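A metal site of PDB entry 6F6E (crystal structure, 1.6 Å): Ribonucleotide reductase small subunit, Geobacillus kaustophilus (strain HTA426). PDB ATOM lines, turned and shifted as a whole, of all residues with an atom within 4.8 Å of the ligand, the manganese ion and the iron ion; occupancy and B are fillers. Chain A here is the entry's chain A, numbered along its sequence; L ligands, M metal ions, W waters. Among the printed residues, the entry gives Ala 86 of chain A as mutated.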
ATOM      1  N   LEU A  75       7.052 -11.476  -6.055  1.00  0.00           N
ATOM      2  CA  LEU A  75       7.693 -12.730  -6.385  1.00  0.00           C
ATOM      3  C   LEU A  75       7.833 -12.896  -7.885  1.00  0.00           C
ATOM      4  O   LEU A  75       8.886 -13.324  -8.368  1.00  0.00           O
ATOM      5  CB  LEU A  75       6.911 -13.903  -5.797  1.00  0.00           C
ATOM      6  CG  LEU A  75       6.901 -14.152  -4.281  1.00  0.00           C
ATOM      7  CD1 LEU A  75       6.265 -15.522  -4.008  1.00  0.00           C
ATOM      8  CD2 LEU A  75       8.283 -14.092  -3.676  1.00  0.00           C
ATOM      9  N   GLY A  78      10.610 -10.892  -9.159  1.00  0.00           N
ATOM     10  CA  GLY A  78      11.934 -11.421  -8.868  1.00  0.00           C
ATOM     11  C   GLY A  78      12.312 -12.549  -9.802  1.00  0.00           C
ATOM     12  O   GLY A  78      13.470 -12.690 -10.195  1.00  0.00           O
ATOM     13  N   PHE A  79      11.325 -13.375 -10.176  1.00  0.00           N
ATOM     14  CA  PHE A  79      11.623 -14.505 -11.050  1.00  0.00           C
ATOM     15  C   PHE A  79      11.794 -14.088 -12.497  1.00  0.00           C
ATOM     16  O   PHE A  79      12.705 -14.576 -13.165  1.00  0.00           O
ATOM     17  CB  PHE A  79      10.510 -15.523 -10.976  1.00  0.00           C
ATOM     18  CG  PHE A  79      10.786 -16.626 -10.028  1.00  0.00           C
ATOM     19  CD1 PHE A  79      11.660 -17.645 -10.377  1.00  0.00           C
ATOM     20  CD2 PHE A  79      10.124 -16.698  -8.805  1.00  0.00           C
ATOM     21  CE1 PHE A  79      11.897 -18.715  -9.488  1.00  0.00           C
ATOM     22  CE2 PHE A  79      10.343 -17.757  -7.921  1.00  0.00           C
ATOM     23  CZ  PHE A  79      11.238 -18.758  -8.264  1.00  0.00           C
ATOM     24  N   GLY A  82      15.071 -12.649 -12.725  1.00  0.00           N
ATOM     25  CA  GLY A  82      16.028 -13.690 -12.430  1.00  0.00           C
ATOM     26  C   GLY A  82      16.270 -14.632 -13.595  1.00  0.00           C
ATOM     27  O   GLY A  82      17.416 -14.970 -13.931  1.00  0.00           O
ATOM     28  N   GLU A  83      15.195 -15.088 -14.235  1.00  0.00           N
ATOM     29  CA  GLU A  83      15.333 -15.978 -15.378  1.00  0.00           C
ATOM     30  C   GLU A  83      15.911 -15.269 -16.591  1.00  0.00           C
ATOM     31  O   GLU A  83      16.594 -15.880 -17.423  1.00  0.00           O
ATOM     32  CB  GLU A  83      13.966 -16.546 -15.750  1.00  0.00           C
ATOM     33  CG  GLU A  83      13.205 -17.183 -14.557  1.00  0.00           C
ATOM     34  CD  GLU A  83      13.839 -18.455 -13.998  1.00  0.00           C
ATOM     35  OE1 GLU A  83      14.768 -18.986 -14.640  1.00  0.00           O
ATOM     36  OE2 GLU A  83      13.416 -18.888 -12.878  1.00  0.00           O
ATOM     37  N   ALA A  86      19.488 -15.064 -15.977  1.00  0.00           N
ATOM     38  CA  ALA A  86      20.050 -16.397 -16.128  1.00  0.00           C
ATOM     39  C   ALA A  86      20.259 -16.740 -17.590  1.00  0.00           C
ATOM     40  O   ALA A  86      21.293 -17.330 -17.963  1.00  0.00           O
ATOM     41  CB  ALA A  86      19.146 -17.428 -15.451  1.00  0.00           C
ATOM     42  N   PHE A 112      20.841 -26.375 -20.551  1.00  0.00           N
ATOM     43  CA  PHE A 112      20.713 -25.380 -19.482  1.00  0.00           C
ATOM     44  C   PHE A 112      20.196 -24.048 -20.033  1.00  0.00           C
ATOM     45  O   PHE A 112      19.190 -23.497 -19.545  1.00  0.00           O
ATOM     46  CB  PHE A 112      22.112 -25.270 -18.856  1.00  0.00           C
ATOM     47  CG  PHE A 112      22.209 -24.505 -17.549  1.00  0.00           C
ATOM     48  CD1 PHE A 112      22.781 -25.100 -16.441  1.00  0.00           C
ATOM     49  CD2 PHE A 112      21.833 -23.182 -17.471  1.00  0.00           C
ATOM     50  CE1 PHE A 112      22.891 -24.431 -15.268  1.00  0.00           C
ATOM     51  CE2 PHE A 112      21.975 -22.486 -16.289  1.00  0.00           C
ATOM     52  CZ  PHE A 112      22.508 -23.117 -15.171  1.00  0.00           C
ATOM     53  N   GLU A 116      16.550 -22.075 -19.511  1.00  0.00           N
ATOM     54  CA  GLU A 116      16.318 -20.746 -18.990  1.00  0.00           C
ATOM     55  C   GLU A 116      15.453 -19.917 -19.937  1.00  0.00           C
ATOM     56  O   GLU A 116      14.640 -19.109 -19.486  1.00  0.00           O
ATOM     57  CB  GLU A 116      17.636 -20.005 -18.751  1.00  0.00           C
ATOM     58  CG  GLU A 116      18.648 -20.707 -17.799  1.00  0.00           C
ATOM     59  CD  GLU A 116      18.115 -20.950 -16.372  1.00  0.00           C
ATOM     60  OE1 GLU A 116      16.940 -20.648 -16.055  1.00  0.00           O
ATOM     61  OE2 GLU A 116      18.933 -21.401 -15.562  1.00  0.00           O
ATOM     62  N   HIS A 119      12.048 -20.697 -19.030  1.00  0.00           N
ATOM     63  CA  HIS A 119      11.627 -20.076 -17.792  1.00  0.00           C
ATOM     64  C   HIS A 119      11.288 -18.599 -17.963  1.00  0.00           C
ATOM     65  O   HIS A 119      10.321 -18.116 -17.381  1.00  0.00           O
ATOM     66  CB  HIS A 119      12.727 -20.206 -16.756  1.00  0.00           C
ATOM     67  CG  HIS A 119      13.130 -21.629 -16.507  1.00  0.00           C
ATOM     68  ND1 HIS A 119      14.204 -21.985 -15.723  1.00  0.00           N
ATOM     69  CD2 HIS A 119      12.614 -22.789 -16.984  1.00  0.00           C
ATOM     70  CE1 HIS A 119      14.353 -23.290 -15.745  1.00  0.00           C
ATOM     71  NE2 HIS A 119      13.385 -23.807 -16.489  1.00  0.00           N
ATOM     72  N   PHE A 149      21.319  -9.482  -8.742  1.00  0.00           N
ATOM     73  CA  PHE A 149      20.919  -9.801 -10.103  1.00  0.00           C
ATOM     74  C   PHE A 149      21.304  -8.748 -11.127  1.00  0.00           C
ATOM     75  O   PHE A 149      21.558  -9.087 -12.293  1.00  0.00           O
ATOM     76  CB  PHE A 149      19.406 -10.010 -10.161  1.00  0.00           C
ATOM     77  CG  PHE A 149      18.957 -11.303  -9.541  1.00  0.00           C
ATOM     78  CD1 PHE A 149      19.012 -12.476 -10.259  1.00  0.00           C
ATOM     79  CD2 PHE A 149      18.512 -11.353  -8.226  1.00  0.00           C
ATOM     80  CE1 PHE A 149      18.622 -13.668  -9.682  1.00  0.00           C
ATOM     81  CE2 PHE A 149      18.120 -12.534  -7.639  1.00  0.00           C
ATOM     82  CZ  PHE A 149      18.163 -13.689  -8.367  1.00  0.00           C
ATOM     83  N   TYR A 176      25.855 -18.107  -9.394  1.00  0.00           N
ATOM     84  CA  TYR A 176      24.774 -18.499 -10.303  1.00  0.00           C
ATOM     85  C   TYR A 176      24.042 -19.723  -9.777  1.00  0.00           C
ATOM     86  O   TYR A 176      22.817 -19.704  -9.597  1.00  0.00           O
ATOM     87  CB  TYR A 176      25.348 -18.765 -11.694  1.00  0.00           C
ATOM     88  CG  TYR A 176      24.384 -18.855 -12.839  1.00  0.00           C
ATOM     89  CD1 TYR A 176      24.493 -18.008 -13.912  1.00  0.00           C
ATOM     90  CD2 TYR A 176      23.415 -19.820 -12.867  1.00  0.00           C
ATOM     91  CE1 TYR A 176      23.637 -18.073 -14.985  1.00  0.00           C
ATOM     92  CE2 TYR A 176      22.539 -19.903 -13.945  1.00  0.00           C
ATOM     93  CZ  TYR A 176      22.667 -19.041 -14.999  1.00  0.00           C
ATOM     94  OH  TYR A 176      21.796 -19.118 -16.083  1.00  0.00           O
ATOM     95  N   VAL A 180      21.871 -18.064  -6.568  1.00  0.00           N
ATOM     96  CA  VAL A 180      20.694 -17.666  -7.339  1.00  0.00           C
ATOM     97  C   VAL A 180      19.732 -18.846  -7.534  1.00  0.00           C
ATOM     98  O   VAL A 180      18.534 -18.741  -7.263  1.00  0.00           O
ATOM     99  CB  VAL A 180      21.113 -17.029  -8.677  1.00  0.00           C
ATOM    100  CG1 VAL A 180      19.911 -16.936  -9.641  1.00  0.00           C
ATOM    101  CG2 VAL A 180      21.732 -15.645  -8.391  1.00  0.00           C
ATOM    102  N   GLU A 181      20.243 -19.994  -8.012  1.00  0.00           N
ATOM    103  CA  GLU A 181      19.369 -21.156  -8.240  1.00  0.00           C
ATOM    104  C   GLU A 181      19.145 -21.935  -6.950  1.00  0.00           C
ATOM    105  O   GLU A 181      18.002 -22.258  -6.592  1.00  0.00           O
ATOM    106  CB  GLU A 181      19.984 -22.076  -9.296  1.00  0.00           C
ATOM    107  CG  GLU A 181      20.072 -21.417 -10.648  1.00  0.00           C
ATOM    108  CD  GLU A 181      20.691 -22.258 -11.683  1.00  0.00           C
ATOM    109  OE1 GLU A 181      21.586 -23.097 -11.389  1.00  0.00           O
ATOM    110  OE2 GLU A 181      20.293 -22.064 -12.842  1.00  0.00           O
ATOM    111  N   LEU A 184      17.914 -18.899  -3.679  1.00  0.00           N
ATOM    112  CA  LEU A 184      16.774 -18.048  -3.962  1.00  0.00           C
ATOM    113  C   LEU A 184      15.722 -18.754  -4.791  1.00  0.00           C
ATOM    114  O   LEU A 184      14.532 -18.784  -4.424  1.00  0.00           O
ATOM    115  CB  LEU A 184      17.257 -16.786  -4.676  1.00  0.00           C
ATOM    116  CG  LEU A 184      17.911 -15.796  -3.723  1.00  0.00           C
ATOM    117  CD1 LEU A 184      18.564 -14.705  -4.582  1.00  0.00           C
ATOM    118  CD2 LEU A 184      16.860 -15.205  -2.787  1.00  0.00           C
ATOM    119  N   ALA A 185      16.108 -19.317  -5.942  1.00  0.00           N
ATOM    120  CA  ALA A 185      15.084 -19.911  -6.799  1.00  0.00           C
ATOM    121  C   ALA A 185      14.345 -21.023  -6.075  1.00  0.00           C
ATOM    122  O   ALA A 185      13.111 -21.097  -6.125  1.00  0.00           O
ATOM    123  CB  ALA A 185      15.683 -20.461  -8.080  1.00  0.00           C
ATOM    124  N   SER A 187      13.910 -21.479  -2.917  1.00  0.00           N
ATOM    125  CA  SER A 187      13.003 -20.940  -1.906  1.00  0.00           C
ATOM    126  C   SER A 187      11.809 -20.253  -2.529  1.00  0.00           C
ATOM    127  O   SER A 187      10.723 -20.263  -1.952  1.00  0.00           O
ATOM    128  CB  SER A 187      13.749 -19.983  -0.985  1.00  0.00           C
ATOM    129  OG  SER A 187      14.830 -20.666  -0.405  1.00  0.00           O
ATOM    130  N   GLY A 188      11.978 -19.674  -3.736  1.00  0.00           N
ATOM    131  CA  GLY A 188      10.848 -19.112  -4.454  1.00  0.00           C
ATOM    132  C   GLY A 188       9.839 -20.138  -4.933  1.00  0.00           C
ATOM    133  O   GLY A 188       8.625 -19.908  -4.872  1.00  0.00           O
ATOM    134  N   THR A 191       7.919 -21.126  -1.727  1.00  0.00           N
ATOM    135  CA  THR A 191       7.043 -20.037  -1.338  1.00  0.00           C
ATOM    136  C   THR A 191       5.816 -19.997  -2.222  1.00  0.00           C
ATOM    137  O   THR A 191       4.693 -19.819  -1.730  1.00  0.00           O
ATOM    138  CB  THR A 191       7.784 -18.708  -1.432  1.00  0.00           C
ATOM    139  OG1 THR A 191       8.916 -18.760  -0.572  1.00  0.00           O
ATOM    140  CG2 THR A 191       6.933 -17.539  -0.999  1.00  0.00           C
ATOM    141  N   LEU A 212       9.670 -25.981 -14.160  1.00  0.00           N
ATOM    142  CA  LEU A 212      10.883 -25.221 -13.937  1.00  0.00           C
ATOM    143  C   LEU A 212      11.699 -25.802 -12.774  1.00  0.00           C
ATOM    144  O   LEU A 212      12.931 -25.928 -12.865  1.00  0.00           O
ATOM    145  CB  LEU A 212      10.459 -23.776 -13.675  1.00  0.00           C
ATOM    146  CG  LEU A 212      11.419 -22.707 -13.349  1.00  0.00           C
ATOM    147  CD1 LEU A 212      10.762 -21.334 -13.649  1.00  0.00           C
ATOM    148  CD2 LEU A 212      11.731 -22.834 -11.906  1.00  0.00           C
ATOM    149  N   GLU A 216      15.583 -27.154 -12.883  1.00  0.00           N
ATOM    150  CA  GLU A 216      16.613 -26.502 -12.084  1.00  0.00           C
ATOM    151  C   GLU A 216      17.378 -27.518 -11.237  1.00  0.00           C
ATOM    152  O   GLU A 216      18.530 -27.277 -10.913  1.00  0.00           O
ATOM    153  CB  GLU A 216      16.016 -25.387 -11.232  1.00  0.00           C
ATOM    154  CG  GLU A 216      15.526 -24.200 -12.127  1.00  0.00           C
ATOM    155  CD  GLU A 216      16.659 -23.495 -12.802  1.00  0.00           C
ATOM    156  OE1 GLU A 216      17.747 -23.478 -12.190  1.00  0.00           O
ATOM    157  OE2 GLU A 216      16.488 -22.959 -13.939  1.00  0.00           O
ATOM    158  N   HIS A 219      20.371 -28.034 -13.135  1.00  0.00           N
ATOM    159  CA  HIS A 219      21.239 -26.856 -13.137  1.00  0.00           C
ATOM    160  C   HIS A 219      22.079 -26.821 -11.854  1.00  0.00           C
ATOM    161  O   HIS A 219      23.291 -26.534 -11.881  1.00  0.00           O
ATOM    162  CB  HIS A 219      20.422 -25.584 -13.238  1.00  0.00           C
ATOM    163  CG  HIS A 219      19.627 -25.494 -14.478  1.00  0.00           C
ATOM    164  ND1 HIS A 219      19.079 -24.314 -14.939  1.00  0.00           N
ATOM    165  CD2 HIS A 219      19.303 -26.447 -15.387  1.00  0.00           C
ATOM    166  CE1 HIS A 219      18.393 -24.572 -16.053  1.00  0.00           C
ATOM    167  NE2 HIS A 219      18.539 -25.847 -16.359  1.00  0.00           N
ATOM    168  N   TYR A 255      17.062  -9.405   0.679  1.00  0.00           N
ATOM    169  CA  TYR A 255      15.949  -9.441  -0.262  1.00  0.00           C
ATOM    170  C   TYR A 255      14.790 -10.245   0.327  1.00  0.00           C
ATOM    171  O   TYR A 255      13.633  -9.823   0.223  1.00  0.00           O
ATOM    172  CB  TYR A 255      16.415 -10.014  -1.602  1.00  0.00           C
ATOM    173  CG  TYR A 255      15.314 -10.267  -2.614  1.00  0.00           C
ATOM    174  CD1 TYR A 255      14.546  -9.223  -3.095  1.00  0.00           C
ATOM    175  CD2 TYR A 255      15.050 -11.544  -3.085  1.00  0.00           C
ATOM    176  CE1 TYR A 255      13.538  -9.442  -4.005  1.00  0.00           C
ATOM    177  CE2 TYR A 255      14.028 -11.784  -4.016  1.00  0.00           C
ATOM    178  CZ  TYR A 255      13.279 -10.716  -4.468  1.00  0.00           C
ATOM    179  OH  TYR A 255      12.265 -10.911  -5.394  1.00  0.00           O
ATOM    180  N   VAL A 256      15.088 -11.354   1.012  1.00  0.00           N
ATOM    181  CA  VAL A 256      14.033 -12.131   1.651  1.00  0.00           C
ATOM    182  C   VAL A 256      13.308 -11.296   2.715  1.00  0.00           C
ATOM    183  O   VAL A 256      12.089 -11.383   2.853  1.00  0.00           O
ATOM    184  CB  VAL A 256      14.625 -13.424   2.253  1.00  0.00           C
ATOM    185  CG1 VAL A 256      13.638 -14.112   3.198  1.00  0.00           C
ATOM    186  CG2 VAL A 256      15.012 -14.393   1.119  1.00  0.00           C
ATOM    187  N   LEU A 259      10.877  -8.888   0.802  1.00  0.00           N
ATOM    188  CA  LEU A 259       9.653  -9.571   0.357  1.00  0.00           C
ATOM    189  C   LEU A 259       8.772  -9.932   1.535  1.00  0.00           C
ATOM    190  O   LEU A 259       7.544  -9.872   1.440  1.00  0.00           O
ATOM    191  CB  LEU A 259       9.993 -10.832  -0.418  1.00  0.00           C
ATOM    192  CG  LEU A 259      10.609 -10.607  -1.793  1.00  0.00           C
ATOM    193  CD1 LEU A 259      10.961 -11.976  -2.325  1.00  0.00           C
ATOM    194  CD2 LEU A 259       9.640  -9.873  -2.720  1.00  0.00           C
ATOM    195  N   THR A 260       9.391 -10.364   2.637  1.00  0.00           N
ATOM    196  CA  THR A 260       8.650 -10.692   3.854  1.00  0.00           C
ATOM    197  C   THR A 260       7.909  -9.472   4.374  1.00  0.00           C
ATOM    198  O   THR A 260       6.730  -9.543   4.724  1.00  0.00           O
ATOM    199  CB  THR A 260       9.616 -11.214   4.910  1.00  0.00           C
ATOM    200  OG1 THR A 260       9.896 -12.592   4.628  1.00  0.00           O
ATOM    201  CG2 THR A 260       9.052 -11.087   6.302  1.00  0.00           C
ATOM    202  N   TYR A 279       5.762 -16.520   7.208  1.00  0.00           N
ATOM    203  CA  TYR A 279       6.999 -16.004   6.650  1.00  0.00           C
ATOM    204  C   TYR A 279       8.207 -16.410   7.466  1.00  0.00           C
ATOM    205  O   TYR A 279       9.307 -16.462   6.924  1.00  0.00           O
ATOM    206  CB  TYR A 279       6.960 -14.479   6.538  1.00  0.00           C
ATOM    207  CG  TYR A 279       5.917 -14.028   5.562  1.00  0.00           C
ATOM    208  CD1 TYR A 279       6.128 -14.135   4.205  1.00  0.00           C
ATOM    209  CD2 TYR A 279       4.710 -13.524   6.003  1.00  0.00           C
ATOM    210  CE1 TYR A 279       5.171 -13.747   3.305  1.00  0.00           C
ATOM    211  CE2 TYR A 279       3.739 -13.124   5.120  1.00  0.00           C
ATOM    212  CZ  TYR A 279       3.984 -13.228   3.766  1.00  0.00           C
ATOM    213  OH  TYR A 279       3.010 -12.845   2.879  1.00  0.00           O
ATOM    214  N   LEU A 282       9.135 -19.596   5.938  1.00  0.00           N
ATOM    215  CA  LEU A 282       9.775 -19.328   4.656  1.00  0.00           C
ATOM    216  C   LEU A 282      11.209 -18.855   4.860  1.00  0.00           C
ATOM    217  O   LEU A 282      12.152 -19.420   4.306  1.00  0.00           O
ATOM    218  CB  LEU A 282       8.986 -18.291   3.864  1.00  0.00           C
ATOM    219  CG  LEU A 282       7.576 -18.732   3.479  1.00  0.00           C
ATOM    220  CD1 LEU A 282       6.820 -17.551   2.853  1.00  0.00           C
ATOM    221  CD2 LEU A 282       7.588 -19.951   2.549  1.00  0.00           C
ATOM    222  N   VAL A 286      14.782 -20.559   3.467  1.00  0.00           N
ATOM    223  CA  VAL A 286      15.925 -19.929   2.809  1.00  0.00           C
ATOM    224  C   VAL A 286      17.217 -20.272   3.543  1.00  0.00           C
ATOM    225  O   VAL A 286      18.225 -20.644   2.927  1.00  0.00           O
ATOM    226  CB  VAL A 286      15.735 -18.417   2.706  1.00  0.00           C
ATOM    227  CG1 VAL A 286      16.923 -17.778   1.994  1.00  0.00           C
ATOM    228  CG2 VAL A 286      14.468 -18.077   1.958  1.00  0.00           C
HETATM  229  C1  LIG L   1      18.150 -19.545 -12.818  1.00  0.00           C
HETATM  230  O1  LIG L   1      17.551 -20.587 -13.174  1.00  0.00           O
HETATM  231  O2  LIG L   1      19.386 -19.383 -12.664  1.00  0.00           O
HETATM  232  C2  LIG L   1      17.312 -18.242 -12.458  1.00  0.00           C
HETATM  233  C3  LIG L   1      16.588 -18.260 -11.107  1.00  0.00           C
HETATM  234  C4  LIG L   1      16.001 -16.916 -10.728  1.00  0.00           C
HETATM  235  C5  LIG L   1      15.232 -16.913  -9.345  1.00  0.00           C
HETATM  236  C6  LIG L   1      15.143 -15.522  -8.711  1.00  0.00           C
HETATM  237  C7  LIG L   1      13.803 -15.035  -8.040  1.00  0.00           C
HETATM  238  C8  LIG L   1      13.265 -15.897  -6.960  1.00  0.00           C
HETATM  239  C9  LIG L   1      12.459 -15.148  -5.821  1.00  0.00           C
HETATM  240  C10 LIG L   1      12.872 -15.731  -4.478  1.00  0.00           C
HETATM  241  C11 LIG L   1      11.923 -15.587  -3.296  1.00  0.00           C
HETATM  242  C12 LIG L   1      12.644 -15.986  -1.988  1.00  0.00           C
HETATM  243  C13 LIG L   1      11.734 -16.478  -0.824  1.00  0.00           C
HETATM  244  C14 LIG L   1      11.099 -15.330  -0.032  1.00  0.00           C
HETATM  245  C15 LIG L   1      10.383 -15.761   1.262  1.00  0.00           C
HETATM  246  C16 LIG L   1       9.467 -14.685   1.799  1.00  0.00           C
HETATM  247 MN    MN M   1      15.619 -20.946 -14.455  1.00  0.00          MN
HETATM  248 FE    FE M   2      18.699 -22.461 -13.879  1.00  0.00          FE
HETATM  249  O   HOH W   1      14.568 -21.109 -12.502  1.00  0.00           O
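OE1 of Glu 116 binds the manganese ion (2.1 Å). OE1 of Glu 83 binds the manganese ion. A ring nitrogen (ND1) of His 119 binds the manganese ion (2.2 Å). Water W1 binds the manganese ion, at 2.2 Å. The manganese ion is bound by OE2 of Glu 216 (2.3 Å). O1 of the ligand is bound to the manganese ion, at 2.3 Å. The manganese ion has six donor atoms within binding distance.
The iron ion is bound by OE2 of Glu 181 (1.9 Å), OE2 of Glu 116 (2.0 Å), ND1 of His 219 (2.2 Å), OE1 of Glu 216 (2.2 Å), OE2 of Glu 216 (2.3 Å) and O1 of the ligand (2.3 Å). The iron ion has six donor atoms within binding distance.
Residues that only touch the ligand: Leu 75 (3.95 Å), Gly 78 (3.2 Å), Phe 79 (3.6 Å), Gly 82 (3.6 Å), Ala 86 (3.4 Å), Phe 149 (3.5 Å), Tyr 176 (3.4 Å), Val 180 (3.9 Å), Leu 184 (3.5 Å), Ala 185 (3.8 Å), Gly 188 (3.9 Å), Thr 191 (3.6 Å), Leu 259 (3.9 Å), Thr 260 (3.5 Å) and Leu 282 (3.9 Å). Hydrophobic or aromatic side chains that line the ligand: Leu 75, Phe 79, Ala 86, Phe 149, Tyr 176, Val 180, Ala 185, Leu 259 and Leu 282. Within 4 Å of the ligand: Leu 75, Gly 78, Phe 79, Gly 82, Glu 83, Ala 86, Glu 116, Phe 149, Tyr 176, Val 180, Glu 181, Leu 184, Ala 185, Gly 188, Thr 191, Glu 216, Leu 259, Thr 260 and Leu 282.
The side-chain hydroxyl (OG1) of Thr 260 lies within hydrogen-bond range of the backbone carbonyl oxygen (O) of Val 256 (3.1 Å). OH of Tyr 176 is in hydrogen-bond range of O of Ala 86, at 2.6 Å. N of Glu 181 lies within hydrogen-bond range of O of Tyr 176 (3.0 Å). O of Ser 187 sits at hydrogen-bond distance from OG1 of Thr 191 (2.7 Å). The backbone carbonyl oxygen (O) of Val 180 is in hydrogen-bond range of the backbone NH (N) of Ala 185.
Within 4 Å of the iron ion: Glu 116, Glu 181, Glu 216 and His 219. The nearest printed residue that does not touch the iron ion is Phe 112 (4.1 Å).
Four residues have an atom within 4 Å of the manganese ion: Glu 83, Glu 116, His 119 and Glu 216.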
